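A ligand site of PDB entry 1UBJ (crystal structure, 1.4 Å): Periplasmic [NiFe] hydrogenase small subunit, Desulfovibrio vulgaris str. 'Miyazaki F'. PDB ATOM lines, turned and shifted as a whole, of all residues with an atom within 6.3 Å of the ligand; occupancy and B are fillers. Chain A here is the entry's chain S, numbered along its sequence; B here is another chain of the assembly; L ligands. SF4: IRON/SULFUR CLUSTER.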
ATOM      1  N   ALA A  15      -3.217 -11.503 -32.700  1.00  0.00           N
ATOM      2  CA  ALA A  15      -1.918 -12.063 -32.361  1.00  0.00           C
ATOM      3  C   ALA A  15      -2.056 -12.666 -30.969  1.00  0.00           C
ATOM      4  O   ALA A  15      -2.086 -11.940 -29.966  1.00  0.00           O
ATOM      5  CB  ALA A  15      -0.858 -10.959 -32.426  1.00  0.00           C
ATOM      6  N   GLU A  16      -2.160 -13.998 -30.943  1.00  0.00           N
ATOM      7  CA  GLU A  16      -2.603 -14.702 -29.740  1.00  0.00           C
ATOM      8  C   GLU A  16      -2.089 -16.133 -29.711  1.00  0.00           C
ATOM      9  O   GLU A  16      -1.652 -16.619 -30.758  1.00  0.00           O
ATOM     10  CB  GLU A  16      -4.141 -14.734 -29.703  1.00  0.00           C
ATOM     11  CG  GLU A  16      -4.906 -15.090 -30.974  1.00  0.00           C
ATOM     12  CD  GLU A  16      -5.056 -16.558 -31.293  1.00  0.00           C
ATOM     13  OE1 GLU A  16      -5.262 -17.385 -30.363  1.00  0.00           O
ATOM     14  OE2 GLU A  16      -4.993 -16.955 -32.483  1.00  0.00           O
ATOM     15  N   CYS A  17      -2.122 -16.733 -28.522  1.00  0.00           N
ATOM     16  CA  CYS A  17      -1.632 -18.107 -28.401  1.00  0.00           C
ATOM     17  C   CYS A  17      -2.748 -19.118 -28.228  1.00  0.00           C
ATOM     18  O   CYS A  17      -2.484 -20.320 -28.175  1.00  0.00           O
ATOM     19  CB  CYS A  17      -0.681 -18.178 -27.212  1.00  0.00           C
ATOM     20  SG  CYS A  17      -1.550 -18.304 -25.611  1.00  0.00           S
ATOM     21  N   THR A  18      -3.971 -18.624 -28.156  1.00  0.00           N
ATOM     22  CA  THR A  18      -5.203 -19.423 -28.066  1.00  0.00           C
ATOM     23  C   THR A  18      -5.404 -19.891 -26.630  1.00  0.00           C
ATOM     24  O   THR A  18      -6.348 -20.598 -26.329  1.00  0.00           O
ATOM     25  CB  THR A  18      -5.224 -20.530 -29.139  1.00  0.00           C
ATOM     26  OG1 THR A  18      -4.954 -19.919 -30.420  1.00  0.00           O
ATOM     27  CG2 THR A  18      -6.604 -21.172 -29.311  1.00  0.00           C
ATOM     28  N   GLY A  19      -4.508 -19.467 -25.724  1.00  0.00           N
ATOM     29  CA  GLY A  19      -4.776 -19.794 -24.312  1.00  0.00           C
ATOM     30  C   GLY A  19      -6.018 -19.074 -23.777  1.00  0.00           C
ATOM     31  O   GLY A  19      -6.717 -19.657 -22.921  1.00  0.00           O
ATOM     32  N   CYS A  20      -6.286 -17.864 -24.252  1.00  0.00           N
ATOM     33  CA  CYS A  20      -7.541 -17.255 -23.782  1.00  0.00           C
ATOM     34  C   CYS A  20      -8.749 -18.032 -24.270  1.00  0.00           C
ATOM     35  O   CYS A  20      -9.718 -18.291 -23.539  1.00  0.00           O
ATOM     36  CB  CYS A  20      -7.576 -15.783 -24.252  1.00  0.00           C
ATOM     37  SG  CYS A  20      -6.423 -14.770 -23.297  1.00  0.00           S
ATOM     38  N   SER A  21      -8.754 -18.467 -25.552  1.00  0.00           N
ATOM     39  CA  SER A  21      -9.852 -19.300 -26.012  1.00  0.00           C
ATOM     40  C   SER A  21     -10.014 -20.550 -25.152  1.00  0.00           C
ATOM     41  O   SER A  21     -11.149 -20.936 -24.808  1.00  0.00           O
ATOM     42  CB  SER A  21      -9.638 -19.793 -27.441  1.00  0.00           C
ATOM     43  OG  SER A  21      -9.933 -18.771 -28.382  1.00  0.00           O
ATOM     44  N   GLU A  75      -9.509 -11.708 -28.707  1.00  0.00           N
ATOM     45  CA  GLU A  75      -8.302 -12.340 -28.168  1.00  0.00           C
ATOM     46  C   GLU A  75      -7.092 -11.944 -29.002  1.00  0.00           C
ATOM     47  O   GLU A  75      -7.156 -12.017 -30.247  1.00  0.00           O
ATOM     48  CB  GLU A  75      -8.542 -13.870 -28.145  1.00  0.00           C
ATOM     49  CG  GLU A  75      -7.328 -14.678 -27.685  1.00  0.00           C
ATOM     50  CD  GLU A  75      -7.614 -16.167 -27.583  1.00  0.00           C
ATOM     51  OE1 GLU A  75      -6.758 -16.946 -27.128  1.00  0.00           O
ATOM     52  OE2 GLU A  75      -8.792 -16.511 -27.953  1.00  0.00           O
ATOM     53  N   GLY A  76      -6.006 -11.506 -28.369  1.00  0.00           N
ATOM     54  CA  GLY A  76      -4.750 -11.232 -29.053  1.00  0.00           C
ATOM     55  C   GLY A  76      -4.566  -9.745 -29.269  1.00  0.00           C
ATOM     56  O   GLY A  76      -5.527  -8.972 -29.385  1.00  0.00           O
ATOM     57  N   GLY A  77      -3.279  -9.390 -29.363  1.00  0.00           N
ATOM     58  CA  GLY A  77      -2.905  -8.016 -29.693  1.00  0.00           C
ATOM     59  C   GLY A  77      -3.033  -7.761 -31.190  1.00  0.00           C
ATOM     60  O   GLY A  77      -3.077  -8.696 -32.004  1.00  0.00           O
ATOM     61  N   TYR A 111     -10.290  -9.623 -24.265  1.00  0.00           N
ATOM     62  CA  TYR A 111     -10.148 -10.769 -23.352  1.00  0.00           C
ATOM     63  C   TYR A 111      -8.699 -11.259 -23.407  1.00  0.00           C
ATOM     64  O   TYR A 111      -8.229 -11.731 -24.461  1.00  0.00           O
ATOM     65  CB  TYR A 111     -11.120 -11.870 -23.741  1.00  0.00           C
ATOM     66  CG  TYR A 111     -11.106 -13.008 -22.738  1.00  0.00           C
ATOM     67  CD1 TYR A 111     -11.419 -12.772 -21.387  1.00  0.00           C
ATOM     68  CD2 TYR A 111     -10.754 -14.296 -23.114  1.00  0.00           C
ATOM     69  CE1 TYR A 111     -11.395 -13.829 -20.451  1.00  0.00           C
ATOM     70  CE2 TYR A 111     -10.744 -15.297 -22.180  1.00  0.00           C
ATOM     71  CZ  TYR A 111     -11.049 -15.095 -20.842  1.00  0.00           C
ATOM     72  OH  TYR A 111     -11.012 -16.140 -19.957  1.00  0.00           O
ATOM     73  N   GLY A 112      -7.971 -11.089 -22.289  1.00  0.00           N
ATOM     74  CA  GLY A 112      -6.618 -11.473 -22.127  1.00  0.00           C
ATOM     75  C   GLY A 112      -5.700 -10.257 -22.254  1.00  0.00           C
ATOM     76  O   GLY A 112      -5.985  -9.316 -22.985  1.00  0.00           O
ATOM     77  N   THR A 113      -4.595 -10.281 -21.519  1.00  0.00           N
ATOM     78  CA  THR A 113      -3.633  -9.194 -21.517  1.00  0.00           C
ATOM     79  C   THR A 113      -3.139  -8.839 -22.915  1.00  0.00           C
ATOM     80  O   THR A 113      -2.796  -7.674 -23.126  1.00  0.00           O
ATOM     81  CB  THR A 113      -2.437  -9.607 -20.631  1.00  0.00           C
ATOM     82  OG1 THR A 113      -3.024  -9.693 -19.316  1.00  0.00           O
ATOM     83  CG2 THR A 113      -1.305  -8.589 -20.606  1.00  0.00           C
ATOM     84  N   CYS A 114      -3.044  -9.790 -23.822  1.00  0.00           N
ATOM     85  CA  CYS A 114      -2.665  -9.370 -25.194  1.00  0.00           C
ATOM     86  C   CYS A 114      -3.712  -8.410 -25.770  1.00  0.00           C
ATOM     87  O   CYS A 114      -3.321  -7.332 -26.267  1.00  0.00           O
ATOM     88  CB  CYS A 114      -2.475 -10.530 -26.163  1.00  0.00           C
ATOM     89  SG  CYS A 114      -1.196 -11.742 -25.676  1.00  0.00           S
ATOM     90  N   ALA A 115      -4.987  -8.807 -25.782  1.00  0.00           N
ATOM     91  CA  ALA A 115      -5.991  -7.894 -26.314  1.00  0.00           C
ATOM     92  C   ALA A 115      -6.156  -6.653 -25.455  1.00  0.00           C
ATOM     93  O   ALA A 115      -6.447  -5.556 -25.984  1.00  0.00           O
ATOM     94  CB  ALA A 115      -7.338  -8.623 -26.434  1.00  0.00           C
ATOM     95  N   GLY A 119       0.354  -7.395 -24.567  1.00  0.00           N
ATOM     96  CA  GLY A 119       0.733  -8.780 -24.276  1.00  0.00           C
ATOM     97  C   GLY A 119       2.141  -9.167 -24.714  1.00  0.00           C
ATOM     98  O   GLY A 119       3.010  -8.336 -24.958  1.00  0.00           O
ATOM     99  N   VAL A 120       2.303 -10.513 -24.804  1.00  0.00           N
ATOM    100  CA  VAL A 120       3.650 -11.086 -24.964  1.00  0.00           C
ATOM    101  C   VAL A 120       4.307 -10.580 -26.234  1.00  0.00           C
ATOM    102  O   VAL A 120       5.529 -10.261 -26.224  1.00  0.00           O
ATOM    103  CB  VAL A 120       3.587 -12.627 -24.874  1.00  0.00           C
ATOM    104  CG1 VAL A 120       2.912 -13.272 -26.089  1.00  0.00           C
ATOM    105  CG2 VAL A 120       4.975 -13.228 -24.683  1.00  0.00           C
ATOM    106  N   GLN A 121       3.617 -10.474 -27.361  1.00  0.00           N
ATOM    107  CA  GLN A 121       4.319 -10.026 -28.579  1.00  0.00           C
ATOM    108  C   GLN A 121       4.596  -8.519 -28.537  1.00  0.00           C
ATOM    109  O   GLN A 121       5.397  -7.990 -29.370  1.00  0.00           O
ATOM    110  CB  GLN A 121       3.520 -10.403 -29.828  1.00  0.00           C
ATOM    111  CG  GLN A 121       2.100  -9.800 -29.850  1.00  0.00           C
ATOM    112  CD  GLN A 121       1.133 -10.730 -29.136  1.00  0.00           C
ATOM    113  OE1 GLN A 121       1.170 -11.937 -29.357  1.00  0.00           O
ATOM    114  NE2 GLN A 121       0.274 -10.180 -28.286  1.00  0.00           N
ATOM    115  N   GLY A 149      -5.267 -10.777 -17.812  1.00  0.00           N
ATOM    116  CA  GLY A 149      -4.754 -12.057 -17.294  1.00  0.00           C
ATOM    117  C   GLY A 149      -4.192 -12.819 -18.512  1.00  0.00           C
ATOM    118  O   GLY A 149      -4.631 -12.586 -19.646  1.00  0.00           O
ATOM    119  N   CYS A 150      -3.342 -13.796 -18.226  1.00  0.00           N
ATOM    120  CA  CYS A 150      -2.627 -14.460 -19.314  1.00  0.00           C
ATOM    121  C   CYS A 150      -2.612 -15.966 -19.128  1.00  0.00           C
ATOM    122  O   CYS A 150      -1.572 -16.585 -18.848  1.00  0.00           O
ATOM    123  CB  CYS A 150      -1.206 -13.852 -19.425  1.00  0.00           C
ATOM    124  SG  CYS A 150      -0.294 -14.291 -20.904  1.00  0.00           S
ATOM    125  N   PRO A 151      -3.768 -16.623 -19.309  1.00  0.00           N
ATOM    126  CA  PRO A 151      -5.064 -16.031 -19.653  1.00  0.00           C
ATOM    127  C   PRO A 151      -5.864 -15.584 -18.426  1.00  0.00           C
ATOM    128  O   PRO A 151      -5.511 -15.903 -17.266  1.00  0.00           O
ATOM    129  CB  PRO A 151      -5.800 -17.193 -20.315  1.00  0.00           C
ATOM    130  CG  PRO A 151      -5.287 -18.422 -19.569  1.00  0.00           C
ATOM    131  CD  PRO A 151      -3.824 -18.123 -19.265  1.00  0.00           C
ATOM    132  N   PRO A 152      -6.924 -14.801 -18.613  1.00  0.00           N
ATOM    133  CA  PRO A 152      -7.722 -14.376 -17.482  1.00  0.00           C
ATOM    134  C   PRO A 152      -8.459 -15.578 -16.885  1.00  0.00           C
ATOM    135  O   PRO A 152      -8.547 -16.647 -17.493  1.00  0.00           O
ATOM    136  CB  PRO A 152      -8.792 -13.438 -18.093  1.00  0.00           C
ATOM    137  CG  PRO A 152      -8.208 -13.060 -19.442  1.00  0.00           C
ATOM    138  CD  PRO A 152      -7.464 -14.306 -19.902  1.00  0.00           C
ATOM    139  N   TRP A 258       5.385  -8.139 -19.081  1.00  0.00           N
ATOM    140  CA  TRP A 258       6.570  -8.864 -19.550  1.00  0.00           C
ATOM    141  C   TRP A 258       7.838  -8.025 -19.317  1.00  0.00           C
ATOM    142  O   TRP A 258       8.941  -8.561 -19.146  1.00  0.00           O
ATOM    143  CB  TRP A 258       6.416  -9.205 -21.033  1.00  0.00           C
ATOM    144  CG  TRP A 258       5.219 -10.090 -21.247  1.00  0.00           C
ATOM    145  CD1 TRP A 258       3.980  -9.740 -21.710  1.00  0.00           C
ATOM    146  CD2 TRP A 258       5.203 -11.486 -20.965  1.00  0.00           C
ATOM    147  NE1 TRP A 258       3.177 -10.862 -21.749  1.00  0.00           N
ATOM    148  CE2 TRP A 258       3.904 -11.929 -21.303  1.00  0.00           C
ATOM    149  CE3 TRP A 258       6.148 -12.403 -20.479  1.00  0.00           C
ATOM    150  CZ2 TRP A 258       3.515 -13.280 -21.150  1.00  0.00           C
ATOM    151  CZ3 TRP A 258       5.752 -13.731 -20.342  1.00  0.00           C
ATOM    152  CH2 TRP A 258       4.444 -14.154 -20.671  1.00  0.00           C
ATOM    153  N   ARG B  41       4.848 -13.410 -34.398  1.00  0.00           N
ATOM    154  CA  ARG B  41       4.960 -12.694 -33.135  1.00  0.00           C
ATOM    155  C   ARG B  41       6.418 -12.404 -32.828  1.00  0.00           C
ATOM    156  O   ARG B  41       6.667 -11.305 -32.317  1.00  0.00           O
ATOM    157  CB  ARG B  41       4.286 -13.435 -31.982  1.00  0.00           C
ATOM    158  CG  ARG B  41       2.791 -13.419 -32.162  1.00  0.00           C
ATOM    159  CD  ARG B  41       2.031 -14.272 -31.138  1.00  0.00           C
ATOM    160  NE  ARG B  41       2.429 -15.666 -31.276  1.00  0.00           N
ATOM    161  CZ  ARG B  41       2.455 -16.622 -30.360  1.00  0.00           C
ATOM    162  NH1 ARG B  41       2.035 -16.396 -29.120  1.00  0.00           N
ATOM    163  NH2 ARG B  41       2.868 -17.832 -30.646  1.00  0.00           N
ATOM    164  N   ARG B  61       3.864 -18.971 -23.647  1.00  0.00           N
ATOM    165  CA  ARG B  61       2.874 -18.209 -24.393  1.00  0.00           C
ATOM    166  C   ARG B  61       3.056 -18.358 -25.897  1.00  0.00           C
ATOM    167  O   ARG B  61       2.349 -17.668 -26.644  1.00  0.00           O
ATOM    168  CB  ARG B  61       2.893 -16.701 -24.040  1.00  0.00           C
ATOM    169  CG  ARG B  61       2.070 -16.483 -22.777  1.00  0.00           C
ATOM    170  CD  ARG B  61       2.651 -17.123 -21.522  1.00  0.00           C
ATOM    171  NE  ARG B  61       1.798 -16.795 -20.383  1.00  0.00           N
ATOM    172  CZ  ARG B  61       2.046 -17.158 -19.143  1.00  0.00           C
ATOM    173  NH1 ARG B  61       3.184 -17.849 -18.904  1.00  0.00           N
ATOM    174  NH2 ARG B  61       1.190 -16.853 -18.150  1.00  0.00           N
ATOM    175  N   GLY B  64      -1.285 -21.748 -26.153  1.00  0.00           N
ATOM    176  CA  GLY B  64      -2.169 -22.130 -25.060  1.00  0.00           C
ATOM    177  C   GLY B  64      -3.007 -23.374 -25.275  1.00  0.00           C
ATOM    178  O   GLY B  64      -3.712 -23.798 -24.353  1.00  0.00           O
ATOM    179  N   PRO B 216      -5.452 -22.784 -18.585  1.00  0.00           N
ATOM    180  CA  PRO B 216      -4.141 -22.812 -19.244  1.00  0.00           C
ATOM    181  C   PRO B 216      -3.013 -22.078 -18.519  1.00  0.00           C
ATOM    182  O   PRO B 216      -3.242 -21.175 -17.664  1.00  0.00           O
ATOM    183  CB  PRO B 216      -4.402 -22.085 -20.577  1.00  0.00           C
ATOM    184  CG  PRO B 216      -5.899 -22.164 -20.753  1.00  0.00           C
ATOM    185  CD  PRO B 216      -6.406 -21.951 -19.345  1.00  0.00           C
ATOM    186  N   HIS B 217      -1.799 -22.475 -18.932  1.00  0.00           N
ATOM    187  CA  HIS B 217      -0.509 -21.866 -18.657  1.00  0.00           C
ATOM    188  C   HIS B 217      -0.092 -22.127 -17.209  1.00  0.00           C
ATOM    189  O   HIS B 217      -0.326 -21.364 -16.275  1.00  0.00           O
ATOM    190  CB  HIS B 217      -0.455 -20.336 -18.976  1.00  0.00           C
ATOM    191  CG  HIS B 217      -0.418 -20.182 -20.481  1.00  0.00           C
ATOM    192  ND1 HIS B 217      -0.650 -19.027 -21.167  1.00  0.00           N
ATOM    193  CD2 HIS B 217      -0.121 -21.112 -21.440  1.00  0.00           C
ATOM    194  CE1 HIS B 217      -0.514 -19.236 -22.496  1.00  0.00           C
ATOM    195  NE2 HIS B 217      -0.172 -20.533 -22.663  1.00  0.00           N
HETATM  196 FE1  SF4 L   1      -2.092 -16.203 -24.874  1.00  0.00          FE
HETATM  197 FE2  SF4 L   1      -2.191 -13.556 -24.943  1.00  0.00          FE
HETATM  198 FE3  SF4 L   1      -1.726 -14.789 -22.661  1.00  0.00          FE
HETATM  199 FE4  SF4 L   1      -4.210 -14.972 -23.780  1.00  0.00          FE
HETATM  200  S1  SF4 L   1      -3.258 -13.042 -22.934  1.00  0.00           S
HETATM  201  S2  SF4 L   1      -2.965 -16.589 -22.794  1.00  0.00           S
HETATM  202  S3  SF4 L   1      -3.641 -14.930 -26.020  1.00  0.00           S
HETATM  203  S4  SF4 L   1      -0.326 -14.848 -24.526  1.00  0.00           S
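The side-chain sulfur of Cys 114 binds an iron atom (FE2) of the ligand, at 2.2 Å. The side-chain sulfur (SG) of Cys 20 binds an iron atom (FE4) of the ligand (2.3 Å). The side-chain sulfur (SG) of Cys 150 binds an iron atom (FE3) of the ligand (2.3 Å). S1 of the ligand sits close to N of Cys 114 (3.4 Å). A ring nitrogen (ND1) of His 217 of chain B lies close to a sulfur (S2) of the ligand (3.7 Å). SG of Cys 17 binds FE1 of the ligand (2.3 Å). The backbone NH of Thr 113 sits close to a sulfur (S1) of the ligand (3.4 Å). S3 of the ligand lies close to N of Cys 17, at 3.4 Å.
A ring nitrogen (ND1) of His 217 of chain B is in hydrogen-bond range of the guanidinium group (NE) of Arg 61 of chain B (3.4 Å). A ring nitrogen (ND1) of His 217 of chain B lies within hydrogen-bond range of the backbone carbonyl oxygen (O) of Cys 150 (3.5 Å). The side-chain sulfur (SG) of Cys 20 lies close to the backbone carbonyl oxygen (O) of Tyr 111 (3.7 Å). OG of Ser 21 is in hydrogen-bond range of OE2 of Glu 75 (2.6 Å). O of Cys 17 is in hydrogen-bond range of N of Gly 64 of chain B (2.8 Å). The backbone carbonyl oxygen (O) of Cys 150 lies within hydrogen-bond range of the guanidinium group (NH2) of Arg 61 of chain B, 2.9 Å away. The side-chain amide nitrogen (NE2) of Gln 121 sits close to the side-chain sulfur (SG) of Cys 114 (3.4 Å). N of Thr 18 lies close to OE1 of Glu 75.
S1 of the ligand lies close to O of Gly 149. N of Pro 151 lies close to S2 of the ligand, at 3.6 Å. Merely in contact with the ligand: Glu 16 (3.7 Å), Gly 19 (3.98 Å), Glu 75 (3.9 Å), Gly 112 (3.8 Å), Val 120 (3.9 Å) and Arg 61 of chain B (3.4 Å). Hydrophobic or aromatic side chains that line the ligand: Val 120, Pro 151 and His 217 of chain B. 14 residues have an atom within 4 Å of the ligand: Glu 16, Cys 17, Gly 19, Cys 20, Glu 75, Gly 112, Thr 113, Cys 114, Val 120, Gly 149, Cys 150, Pro 151, Arg 61 of chain B and His 217 of chain B.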
